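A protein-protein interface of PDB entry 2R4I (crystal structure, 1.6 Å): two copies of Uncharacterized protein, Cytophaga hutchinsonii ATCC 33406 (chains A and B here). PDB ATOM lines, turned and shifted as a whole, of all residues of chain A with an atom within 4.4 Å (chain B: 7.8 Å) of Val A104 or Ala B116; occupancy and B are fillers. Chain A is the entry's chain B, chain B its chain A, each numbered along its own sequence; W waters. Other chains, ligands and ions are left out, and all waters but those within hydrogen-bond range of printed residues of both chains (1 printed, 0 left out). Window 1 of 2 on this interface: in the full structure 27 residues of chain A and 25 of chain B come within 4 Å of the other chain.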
ATOM      1  N   THR A  77       8.345  12.775  29.821  1.00  0.00           N
ATOM      2  CA  THR A  77       8.570  13.549  28.612  1.00  0.00           C
ATOM      3  C   THR A  77       8.483  12.662  27.386  1.00  0.00           C
ATOM      4  O   THR A  77       8.901  11.534  27.403  1.00  0.00           O
ATOM      5  CB  THR A  77       9.922  14.306  28.725  1.00  0.00           C
ATOM      6  OG1 THR A  77       9.855  15.195  29.849  1.00  0.00           O
ATOM      7  CG2 THR A  77      10.261  15.112  27.439  1.00  0.00           C
ATOM      8  N   VAL A  78       7.895  13.187  26.320  1.00  0.00           N
ATOM      9  CA  VAL A  78       7.736  12.478  25.068  1.00  0.00           C
ATOM     10  C   VAL A  78       8.249  13.373  23.935  1.00  0.00           C
ATOM     11  O   VAL A  78       7.872  14.541  23.843  1.00  0.00           O
ATOM     12  CB  VAL A  78       6.289  12.059  24.808  1.00  0.00           C
ATOM     13  CG1 VAL A  78       6.206  11.309  23.468  1.00  0.00           C
ATOM     14  CG2 VAL A  78       5.773  11.184  25.964  1.00  0.00           C
ATOM     15  N   VAL A  79       9.140  12.815  23.124  1.00  0.00           N
ATOM     16  CA  VAL A  79       9.762  13.511  22.018  1.00  0.00           C
ATOM     17  C   VAL A  79       9.055  13.010  20.766  1.00  0.00           C
ATOM     18  O   VAL A  79       8.955  11.791  20.547  1.00  0.00           O
ATOM     19  CB  VAL A  79      11.292  13.249  21.934  1.00  0.00           C
ATOM     20  CG1 VAL A  79      11.921  14.047  20.835  1.00  0.00           C
ATOM     21  CG2 VAL A  79      12.018  13.567  23.287  1.00  0.00           C
ATOM     22  N   ARG A 103       8.526  18.190  18.351  1.00  0.00           N
ATOM     23  CA  ARG A 103       7.815  18.696  19.544  1.00  0.00           C
ATOM     24  C   ARG A 103       8.244  17.888  20.723  1.00  0.00           C
ATOM     25  O   ARG A 103       8.426  16.690  20.606  1.00  0.00           O
ATOM     26  CB  ARG A 103       6.296  18.691  19.465  1.00  0.00           C
ATOM     27  CG  ARG A 103       5.693  19.982  18.928  1.00  0.00           C
ATOM     28  CD  ARG A 103       4.175  19.922  18.957  1.00  0.00           C
ATOM     29  NE  ARG A 103       3.612  19.052  17.905  1.00  0.00           N
ATOM     30  CZ  ARG A 103       3.437  19.413  16.628  1.00  0.00           C
ATOM     31  NH1 ARG A 103       3.806  20.612  16.179  1.00  0.00           N
ATOM     32  NH2 ARG A 103       2.902  18.549  15.779  1.00  0.00           N
ATOM     33  N   VAL A 104       8.396  18.553  21.863  1.00  0.00           N
ATOM     34  CA  VAL A 104       8.706  17.874  23.140  1.00  0.00           C
ATOM     35  C   VAL A 104       7.553  18.205  24.091  1.00  0.00           C
ATOM     36  O   VAL A 104       7.294  19.373  24.353  1.00  0.00           O
ATOM     37  CB  VAL A 104      10.055  18.283  23.724  1.00  0.00           C
ATOM     38  CG1 VAL A 104      10.324  17.524  25.068  1.00  0.00           C
ATOM     39  CG2 VAL A 104      11.154  18.090  22.695  1.00  0.00           C
ATOM     40  N   TRP A 105       6.841  17.154  24.499  1.00  0.00           N
ATOM     41  CA  TRP A 105       5.720  17.209  25.444  1.00  0.00           C
ATOM     42  C   TRP A 105       6.206  16.771  26.828  1.00  0.00           C
ATOM     43  O   TRP A 105       6.980  15.835  26.943  1.00  0.00           O
ATOM     44  CB  TRP A 105       4.595  16.263  25.047  1.00  0.00           C
ATOM     45  CG  TRP A 105       3.840  16.630  23.812  1.00  0.00           C
ATOM     46  CD1 TRP A 105       4.140  16.255  22.531  1.00  0.00           C
ATOM     47  CD2 TRP A 105       2.649  17.416  23.741  1.00  0.00           C
ATOM     48  NE1 TRP A 105       3.218  16.759  21.677  1.00  0.00           N
ATOM     49  CE2 TRP A 105       2.273  17.473  22.379  1.00  0.00           C
ATOM     50  CE3 TRP A 105       1.832  18.064  24.697  1.00  0.00           C
ATOM     51  CZ2 TRP A 105       1.117  18.158  21.945  1.00  0.00           C
ATOM     52  CZ3 TRP A 105       0.678  18.716  24.276  1.00  0.00           C
ATOM     53  CH2 TRP A 105       0.346  18.785  22.910  1.00  0.00           C
ATOM     54  N   LYS A 106       5.732  17.448  27.860  1.00  0.00           N
ATOM     55  CA  LYS A 106       6.071  17.096  29.269  1.00  0.00           C
ATOM     56  C   LYS A 106       4.845  17.242  30.155  1.00  0.00           C
ATOM     57  O   LYS A 106       3.970  18.023  29.877  1.00  0.00           O
ATOM     58  CB  LYS A 106       7.274  17.957  29.740  1.00  0.00           C
ATOM     59  CG  LYS A 106       7.754  17.752  31.202  1.00  0.00           C
ATOM     60  CD  LYS A 106       8.997  18.587  31.435  1.00  0.00           C
ATOM     61  CE  LYS A 106       9.397  18.757  32.887  1.00  0.00           C
ATOM     62  NZ  LYS A 106       9.728  17.498  33.628  1.00  0.00           N
ATOM     63  N   LYS A 113       1.992  19.307  28.187  1.00  0.00           N
ATOM     64  CA  LYS A 113       2.206  20.611  27.569  1.00  0.00           C
ATOM     65  C   LYS A 113       3.467  20.569  26.697  1.00  0.00           C
ATOM     66  O   LYS A 113       4.415  19.837  26.988  1.00  0.00           O
ATOM     67  CB  LYS A 113       2.319  21.716  28.630  1.00  0.00           C
ATOM     68  CG  LYS A 113       1.062  21.891  29.534  1.00  0.00           C
ATOM     69  CD  LYS A 113       1.164  23.097  30.459  1.00  0.00           C
ATOM     70  CE  LYS A 113      -0.031  23.242  31.414  1.00  0.00           C
ATOM     71  NZ  LYS A 113      -1.356  23.228  30.744  1.00  0.00           N
ATOM     72  N   VAL A 114       3.440  21.340  25.621  1.00  0.00           N
ATOM     73  CA  VAL A 114       4.556  21.478  24.697  1.00  0.00           C
ATOM     74  C   VAL A 114       5.581  22.450  25.311  1.00  0.00           C
ATOM     75  O   VAL A 114       5.254  23.620  25.586  1.00  0.00           O
ATOM     76  CB  VAL A 114       4.135  21.986  23.312  1.00  0.00           C
ATOM     77  CG1 VAL A 114       5.344  22.210  22.406  1.00  0.00           C
ATOM     78  CG2 VAL A 114       3.092  21.045  22.684  1.00  0.00           C
ATOM     79  N   ILE A 115       6.805  21.958  25.490  1.00  0.00           N
ATOM     80  CA  ILE A 115       7.930  22.800  26.039  1.00  0.00           C
ATOM     81  C   ILE A 115       8.992  23.249  25.042  1.00  0.00           C
ATOM     82  O   ILE A 115       9.745  24.153  25.341  1.00  0.00           O
ATOM     83  CB  ILE A 115       8.635  22.096  27.228  1.00  0.00           C
ATOM     84  CG1 ILE A 115       9.272  20.757  26.817  1.00  0.00           C
ATOM     85  CG2 ILE A 115       7.647  21.843  28.412  1.00  0.00           C
ATOM     86  CD1 ILE A 115      10.283  20.279  27.925  1.00  0.00           C
ATOM     87  N   ALA A 116       9.016  22.675  23.842  1.00  0.00           N
ATOM     88  CA  ALA A 116      10.021  22.952  22.861  1.00  0.00           C
ATOM     89  C   ALA A 116       9.604  22.361  21.543  1.00  0.00           C
ATOM     90  O   ALA A 116       8.845  21.382  21.488  1.00  0.00           O
ATOM     91  CB  ALA A 116      11.348  22.304  23.270  1.00  0.00           C
ATOM     92  N   HIS B  32      21.365  11.289  25.456  1.00  0.00           N
ATOM     93  CA  HIS B  32      20.462  10.228  25.953  1.00  0.00           C
ATOM     94  C   HIS B  32      20.206   9.180  24.850  1.00  0.00           C
ATOM     95  O   HIS B  32      19.986   9.535  23.672  1.00  0.00           O
ATOM     96  CB  HIS B  32      19.147  10.853  26.435  1.00  0.00           C
ATOM     97  CG  HIS B  32      18.261   9.926  27.220  1.00  0.00           C
ATOM     98  ND1 HIS B  32      17.479   8.974  26.628  1.00  0.00           N
ATOM     99  CD2 HIS B  32      17.952   9.892  28.544  1.00  0.00           C
ATOM    100  CE1 HIS B  32      16.831   8.287  27.555  1.00  0.00           C
ATOM    101  NE2 HIS B  32      17.061   8.862  28.725  1.00  0.00           N
ATOM    102  N   ASP B  34      17.716   7.578  23.939  1.00  0.00           N
ATOM    103  CA  ASP B  34      16.423   7.699  23.272  1.00  0.00           C
ATOM    104  C   ASP B  34      16.120   9.045  22.683  1.00  0.00           C
ATOM    105  O   ASP B  34      14.949   9.371  22.452  1.00  0.00           O
ATOM    106  CB  ASP B  34      15.338   7.291  24.283  1.00  0.00           C
ATOM    107  CG  ASP B  34      15.537   5.876  24.800  1.00  0.00           C
ATOM    108  OD1 ASP B  34      15.954   5.001  24.005  1.00  0.00           O
ATOM    109  OD2 ASP B  34      15.310   5.659  26.021  1.00  0.00           O
ATOM    110  N   LEU B  35      17.148   9.846  22.418  1.00  0.00           N
ATOM    111  CA  LEU B  35      16.904  11.126  21.806  1.00  0.00           C
ATOM    112  C   LEU B  35      16.448  11.016  20.354  1.00  0.00           C
ATOM    113  O   LEU B  35      16.636   9.968  19.688  1.00  0.00           O
ATOM    114  CB  LEU B  35      18.167  11.993  21.832  1.00  0.00           C
ATOM    115  CG  LEU B  35      19.395  11.610  20.989  1.00  0.00           C
ATOM    116  CD1 LEU B  35      19.198  11.994  19.503  1.00  0.00           C
ATOM    117  CD2 LEU B  35      20.722  12.207  21.546  1.00  0.00           C
ATOM    118  N   LEU B  36      15.834  12.096  19.856  1.00  0.00           N
ATOM    119  CA  LEU B  36      15.607  12.290  18.433  1.00  0.00           C
ATOM    120  C   LEU B  36      16.138  13.666  18.050  1.00  0.00           C
ATOM    121  O   LEU B  36      15.940  14.629  18.773  1.00  0.00           O
ATOM    122  CB  LEU B  36      14.132  12.253  18.052  1.00  0.00           C
ATOM    123  CG  LEU B  36      13.374  10.958  18.314  1.00  0.00           C
ATOM    124  CD1 LEU B  36      11.930  11.248  17.962  1.00  0.00           C
ATOM    125  CD2 LEU B  36      14.020   9.779  17.547  1.00  0.00           C
ATOM    126  N   PHE B  37      16.838  13.711  16.916  1.00  0.00           N
ATOM    127  CA  PHE B  37      17.335  14.947  16.344  1.00  0.00           C
ATOM    128  C   PHE B  37      16.746  15.133  14.957  1.00  0.00           C
ATOM    129  O   PHE B  37      16.591  14.175  14.225  1.00  0.00           O
ATOM    130  CB  PHE B  37      18.846  14.909  16.081  1.00  0.00           C
ATOM    131  CG  PHE B  37      19.735  14.966  17.290  1.00  0.00           C
ATOM    132  CD1 PHE B  37      19.492  15.838  18.356  1.00  0.00           C
ATOM    133  CD2 PHE B  37      20.923  14.245  17.292  1.00  0.00           C
ATOM    134  CE1 PHE B  37      20.396  15.905  19.479  1.00  0.00           C
ATOM    135  CE2 PHE B  37      21.825  14.339  18.378  1.00  0.00           C
ATOM    136  CZ  PHE B  37      21.546  15.151  19.457  1.00  0.00           C
ATOM    137  N   ILE B  38      16.388  16.358  14.590  1.00  0.00           N
ATOM    138  CA  ILE B  38      15.988  16.666  13.222  1.00  0.00           C
ATOM    139  C   ILE B  38      17.114  17.510  12.599  1.00  0.00           C
ATOM    140  O   ILE B  38      17.594  18.480  13.207  1.00  0.00           O
ATOM    141  CB  ILE B  38      14.610  17.367  13.156  1.00  0.00           C
ATOM    142  CG1 ILE B  38      13.521  16.390  13.655  1.00  0.00           C
ATOM    143  CG2 ILE B  38      14.337  17.838  11.747  1.00  0.00           C
ATOM    144  CD1 ILE B  38      12.086  16.919  13.639  1.00  0.00           C
ATOM    145  N   THR B  77      14.390  20.204  33.236  1.00  0.00           N
ATOM    146  CA  THR B  77      14.719  20.355  31.835  1.00  0.00           C
ATOM    147  C   THR B  77      15.215  21.769  31.532  1.00  0.00           C
ATOM    148  O   THR B  77      14.698  22.763  32.084  1.00  0.00           O
ATOM    149  CB  THR B  77      13.448  20.058  30.979  1.00  0.00           C
ATOM    150  OG1 THR B  77      12.960  18.757  31.317  1.00  0.00           O
ATOM    151  CG2 THR B  77      13.711  20.100  29.510  1.00  0.00           C
ATOM    152  N   VAL B  78      16.256  21.856  30.698  1.00  0.00           N
ATOM    153  CA  VAL B  78      16.776  23.122  30.144  1.00  0.00           C
ATOM    154  C   VAL B  78      16.572  23.088  28.622  1.00  0.00           C
ATOM    155  O   VAL B  78      17.015  22.170  27.939  1.00  0.00           O
ATOM    156  CB  VAL B  78      18.215  23.385  30.535  1.00  0.00           C
ATOM    157  CG1 VAL B  78      18.664  24.782  30.035  1.00  0.00           C
ATOM    158  CG2 VAL B  78      18.364  23.306  32.035  1.00  0.00           C
ATOM    159  N   VAL B  79      15.847  24.078  28.105  1.00  0.00           N
ATOM    160  CA  VAL B  79      15.575  24.229  26.660  1.00  0.00           C
ATOM    161  C   VAL B  79      16.509  25.367  26.210  1.00  0.00           C
ATOM    162  O   VAL B  79      16.503  26.460  26.804  1.00  0.00           O
ATOM    163  CB  VAL B  79      14.079  24.578  26.373  1.00  0.00           C
ATOM    164  CG1 VAL B  79      13.861  24.734  24.857  1.00  0.00           C
ATOM    165  CG2 VAL B  79      13.124  23.515  26.948  1.00  0.00           C
ATOM    166  N   VAL B  80      17.312  25.086  25.172  1.00  0.00           N
ATOM    167  CA  VAL B  80      18.314  25.988  24.631  1.00  0.00           C
ATOM    168  C   VAL B  80      18.144  26.205  23.138  1.00  0.00           C
ATOM    169  O   VAL B  80      17.921  25.259  22.393  1.00  0.00           O
ATOM    170  CB  VAL B  80      19.714  25.338  24.876  1.00  0.00           C
ATOM    171  CG1 VAL B  80      20.821  25.987  24.143  1.00  0.00           C
ATOM    172  CG2 VAL B  80      19.999  25.300  26.432  1.00  0.00           C
ATOM    173  N   LEU B 102      18.462  23.860  18.393  1.00  0.00           N
ATOM    174  CA  LEU B 102      17.584  23.672  19.518  1.00  0.00           C
ATOM    175  C   LEU B 102      18.101  22.416  20.215  1.00  0.00           C
ATOM    176  O   LEU B 102      18.299  21.402  19.554  1.00  0.00           O
ATOM    177  CB  LEU B 102      16.140  23.426  19.064  1.00  0.00           C
ATOM    178  CG  LEU B 102      15.099  23.177  20.170  1.00  0.00           C
ATOM    179  CD1 LEU B 102      14.930  24.393  21.031  1.00  0.00           C
ATOM    180  CD2 LEU B 102      13.758  22.659  19.568  1.00  0.00           C
ATOM    181  N   ARG B 103      18.266  22.483  21.531  1.00  0.00           N
ATOM    182  CA  ARG B 103      18.554  21.295  22.364  1.00  0.00           C
ATOM    183  C   ARG B 103      17.702  21.317  23.625  1.00  0.00           C
ATOM    184  O   ARG B 103      17.452  22.382  24.230  1.00  0.00           O
ATOM    185  CB  ARG B 103      20.043  21.153  22.705  1.00  0.00           C
ATOM    186  CG  ARG B 103      20.892  20.420  21.648  1.00  0.00           C
ATOM    187  CD  ARG B 103      22.396  20.281  22.054  1.00  0.00           C
ATOM    188  NE  ARG B 103      23.118  21.553  22.008  1.00  0.00           N
ATOM    189  CZ  ARG B 103      23.777  21.986  20.927  1.00  0.00           C
ATOM    190  NH1 ARG B 103      23.749  21.300  19.809  1.00  0.00           N
ATOM    191  NH2 ARG B 103      24.427  23.135  20.976  1.00  0.00           N
ATOM    192  N   VAL B 104      17.211  20.129  24.001  1.00  0.00           N
ATOM    193  CA  VAL B 104      16.479  19.928  25.233  1.00  0.00           C
ATOM    194  C   VAL B 104      17.316  18.970  26.076  1.00  0.00           C
ATOM    195  O   VAL B 104      17.599  17.834  25.667  1.00  0.00           O
ATOM    196  CB  VAL B 104      15.065  19.381  24.974  1.00  0.00           C
ATOM    197  CG1 VAL B 104      14.293  19.208  26.312  1.00  0.00           C
ATOM    198  CG2 VAL B 104      14.352  20.297  24.001  1.00  0.00           C
ATOM    199  N   TRP B 105      17.698  19.448  27.267  1.00  0.00           N
ATOM    200  CA  TRP B 105      18.482  18.718  28.204  1.00  0.00           C
ATOM    201  C   TRP B 105      17.597  18.328  29.398  1.00  0.00           C
ATOM    202  O   TRP B 105      16.857  19.156  29.920  1.00  0.00           O
ATOM    203  CB  TRP B 105      19.611  19.568  28.755  1.00  0.00           C
ATOM    204  CG  TRP B 105      20.677  19.966  27.777  1.00  0.00           C
ATOM    205  CD1 TRP B 105      20.655  21.046  26.954  1.00  0.00           C
ATOM    206  CD2 TRP B 105      21.962  19.346  27.599  1.00  0.00           C
ATOM    207  NE1 TRP B 105      21.818  21.139  26.248  1.00  0.00           N
ATOM    208  CE2 TRP B 105      22.648  20.110  26.613  1.00  0.00           C
ATOM    209  CE3 TRP B 105      22.599  18.220  28.157  1.00  0.00           C
ATOM    210  CZ2 TRP B 105      23.948  19.781  26.185  1.00  0.00           C
ATOM    211  CZ3 TRP B 105      23.896  17.893  27.737  1.00  0.00           C
ATOM    212  CH2 TRP B 105      24.547  18.672  26.741  1.00  0.00           C
ATOM    213  N   LYS B 106      17.765  17.106  29.889  1.00  0.00           N
ATOM    214  CA  LYS B 106      17.053  16.603  31.058  1.00  0.00           C
ATOM    215  C   LYS B 106      18.041  16.072  32.098  1.00  0.00           C
ATOM    216  O   LYS B 106      19.010  15.383  31.772  1.00  0.00           O
ATOM    217  CB  LYS B 106      16.105  15.479  30.627  1.00  0.00           C
ATOM    218  CG  LYS B 106      15.097  14.957  31.691  1.00  0.00           C
ATOM    219  CD  LYS B 106      14.272  13.797  31.170  1.00  0.00           C
ATOM    220  CE  LYS B 106      13.188  13.321  32.152  1.00  0.00           C
ATOM    221  NZ  LYS B 106      12.272  14.459  32.491  1.00  0.00           N
ATOM    222  N   LYS B 113      21.578  15.332  30.220  1.00  0.00           N
ATOM    223  CA  LYS B 113      21.645  14.644  28.927  1.00  0.00           C
ATOM    224  C   LYS B 113      20.682  15.258  27.906  1.00  0.00           C
ATOM    225  O   LYS B 113      19.539  15.626  28.197  1.00  0.00           O
ATOM    226  CB  LYS B 113      21.290  13.143  29.096  1.00  0.00           C
ATOM    227  CG  LYS B 113      22.116  12.355  30.041  1.00  0.00           C
ATOM    228  CD  LYS B 113      21.605  10.927  30.236  1.00  0.00           C
ATOM    229  CE  LYS B 113      22.444  10.162  31.289  1.00  0.00           C
ATOM    230  NZ  LYS B 113      23.888  10.033  30.883  1.00  0.00           N
ATOM    231  N   VAL B 114      21.129  15.338  26.640  1.00  0.00           N
ATOM    232  CA  VAL B 114      20.297  15.781  25.556  1.00  0.00           C
ATOM    233  C   VAL B 114      19.275  14.719  25.189  1.00  0.00           C
ATOM    234  O   VAL B 114      19.643  13.583  24.886  1.00  0.00           O
ATOM    235  CB  VAL B 114      21.137  16.062  24.276  1.00  0.00           C
ATOM    236  CG1 VAL B 114      20.237  16.558  23.120  1.00  0.00           C
ATOM    237  CG2 VAL B 114      22.248  17.105  24.540  1.00  0.00           C
ATOM    238  N   ILE B 115      18.007  15.071  25.264  1.00  0.00           N
ATOM    239  CA  ILE B 115      16.908  14.184  24.872  1.00  0.00           C
ATOM    240  C   ILE B 115      16.234  14.509  23.518  1.00  0.00           C
ATOM    241  O   ILE B 115      15.465  13.715  23.037  1.00  0.00           O
ATOM    242  CB  ILE B 115      15.823  14.099  25.993  1.00  0.00           C
ATOM    243  CG1 ILE B 115      15.253  15.487  26.286  1.00  0.00           C
ATOM    244  CG2 ILE B 115      16.365  13.439  27.264  1.00  0.00           C
ATOM    245  CD1 ILE B 115      13.887  15.375  26.932  1.00  0.00           C
ATOM    246  N   ALA B 116      16.482  15.706  22.960  1.00  0.00           N
ATOM    247  CA  ALA B 116      15.858  16.158  21.742  1.00  0.00           C
ATOM    248  C   ALA B 116      16.604  17.337  21.183  1.00  0.00           C
ATOM    249  O   ALA B 116      17.223  18.098  21.941  1.00  0.00           O
ATOM    250  CB  ALA B 116      14.397  16.535  22.017  1.00  0.00           C
ATOM    251  N   GLY B 117      16.579  17.483  19.867  1.00  0.00           N
ATOM    252  CA  GLY B 117      17.086  18.675  19.275  1.00  0.00           C
ATOM    253  C   GLY B 117      16.835  18.792  17.804  1.00  0.00           C
ATOM    254  O   GLY B 117      16.349  17.840  17.149  1.00  0.00           O
ATOM    255  N   SER B 118      17.196  19.958  17.271  1.00  0.00           N
ATOM    256  CA  SER B 118      17.143  20.169  15.846  1.00  0.00           C
ATOM    257  C   SER B 118      18.189  21.190  15.404  1.00  0.00           C
ATOM    258  O   SER B 118      18.735  21.942  16.216  1.00  0.00           O
ATOM    259  CB  SER B 118      15.753  20.579  15.371  1.00  0.00           C
ATOM    260  OG  SER B 118      15.414  21.820  15.933  1.00  0.00           O
HETATM  261  O   HOH W   1      12.309  16.336  30.317  1.00  0.00           O
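Water W1 lies within hydrogen-bond range of the side-chain hydroxyl (OG1) of Thr B77 (2.7 Å), the side-chain hydroxyl (OG1) of Thr A77 (2.7 Å) and the side-chain amino group (NZ) of Lys B106 (2.9 Å).
The backbone NH (N) of Val A104 is in hydrogen-bond range of the backbone carbonyl oxygen (O) of Ala A116, at 2.9 Å. O of Leu B36 lies within hydrogen-bond range of N of Gly B117 (3.1 Å). O of Val A104 is in hydrogen-bond range of N of Ile A115 (2.9 Å). The backbone carbonyl oxygen of Val B104 sits at hydrogen-bond distance from the backbone NH of Ile B115, 2.8 Å away. The backbone carbonyl oxygen (O) of Lys A113 lies within hydrogen-bond range of the backbone NH (N) of Lys A106 (2.9 Å). The backbone carbonyl oxygen (O) of Ala B116 is in hydrogen-bond range of the backbone NH (N) of Val B104.
Thr A77 touches Ile B115, and with the chains exchanged Ile A115 touches Thr B77. Val A79 touches Ile B115, and with the chains exchanged Ile A115 touches Val B79. Val A79 touches Ala B116, and with the chains exchanged Ala A116 touches Val B79. Val A104 touches Ala B116, and with the chains exchanged Ala A116 touches Val B104. 11 positions are printed for both chains.
Printed residues of chain B within 4 Å of Val A79: Leu B36, Ile B115 and Ala B116. Val A104 touches just one residue of chain B: Ala B116. Of the printed residues of chain A, Leu B36 touches Val A79. Of the printed residues of chain A, Thr B77 touches Lys A106 (3.9 Å) and Ile A115 (3.8 Å). Of chain A, only Val A79 (3.7 Å) and Val A104 (3.7 Å) come within 4 Å of Ala B116. The nearest printed residue of chain B that does not touch Val A79 is Asp B34 (5.2 Å).
Among the printed residues, pairs that only touch across the chains: Thr A77 with Lys B106, Thr A77 with Ile B115, Val A79 with Leu B36, Val A79 with Ile B115, Val A79 with Ala B116, Val A104 with Ala B116, Lys A106 with Thr B77, Ile A115 with Thr B77, Ile A115 with Val B79, Ala A116 with Val B79 and Ala A116 with Val B104.
Of the 21 printed residues of chain B, 7 touch a printed residue of chain A. Hydrophobic or aromatic side chains of chain A that line the printed part of chain B: Val A79, Val A104, Ile A115 and Ala A116. Along chain A the printed residues that touch a printed residue of chain B span positions 77 to 116. Among the printed residues, no Asp or Glu carboxylate lies within 4 Å of a Lys or Arg side-chain nitrogen of the other chain.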
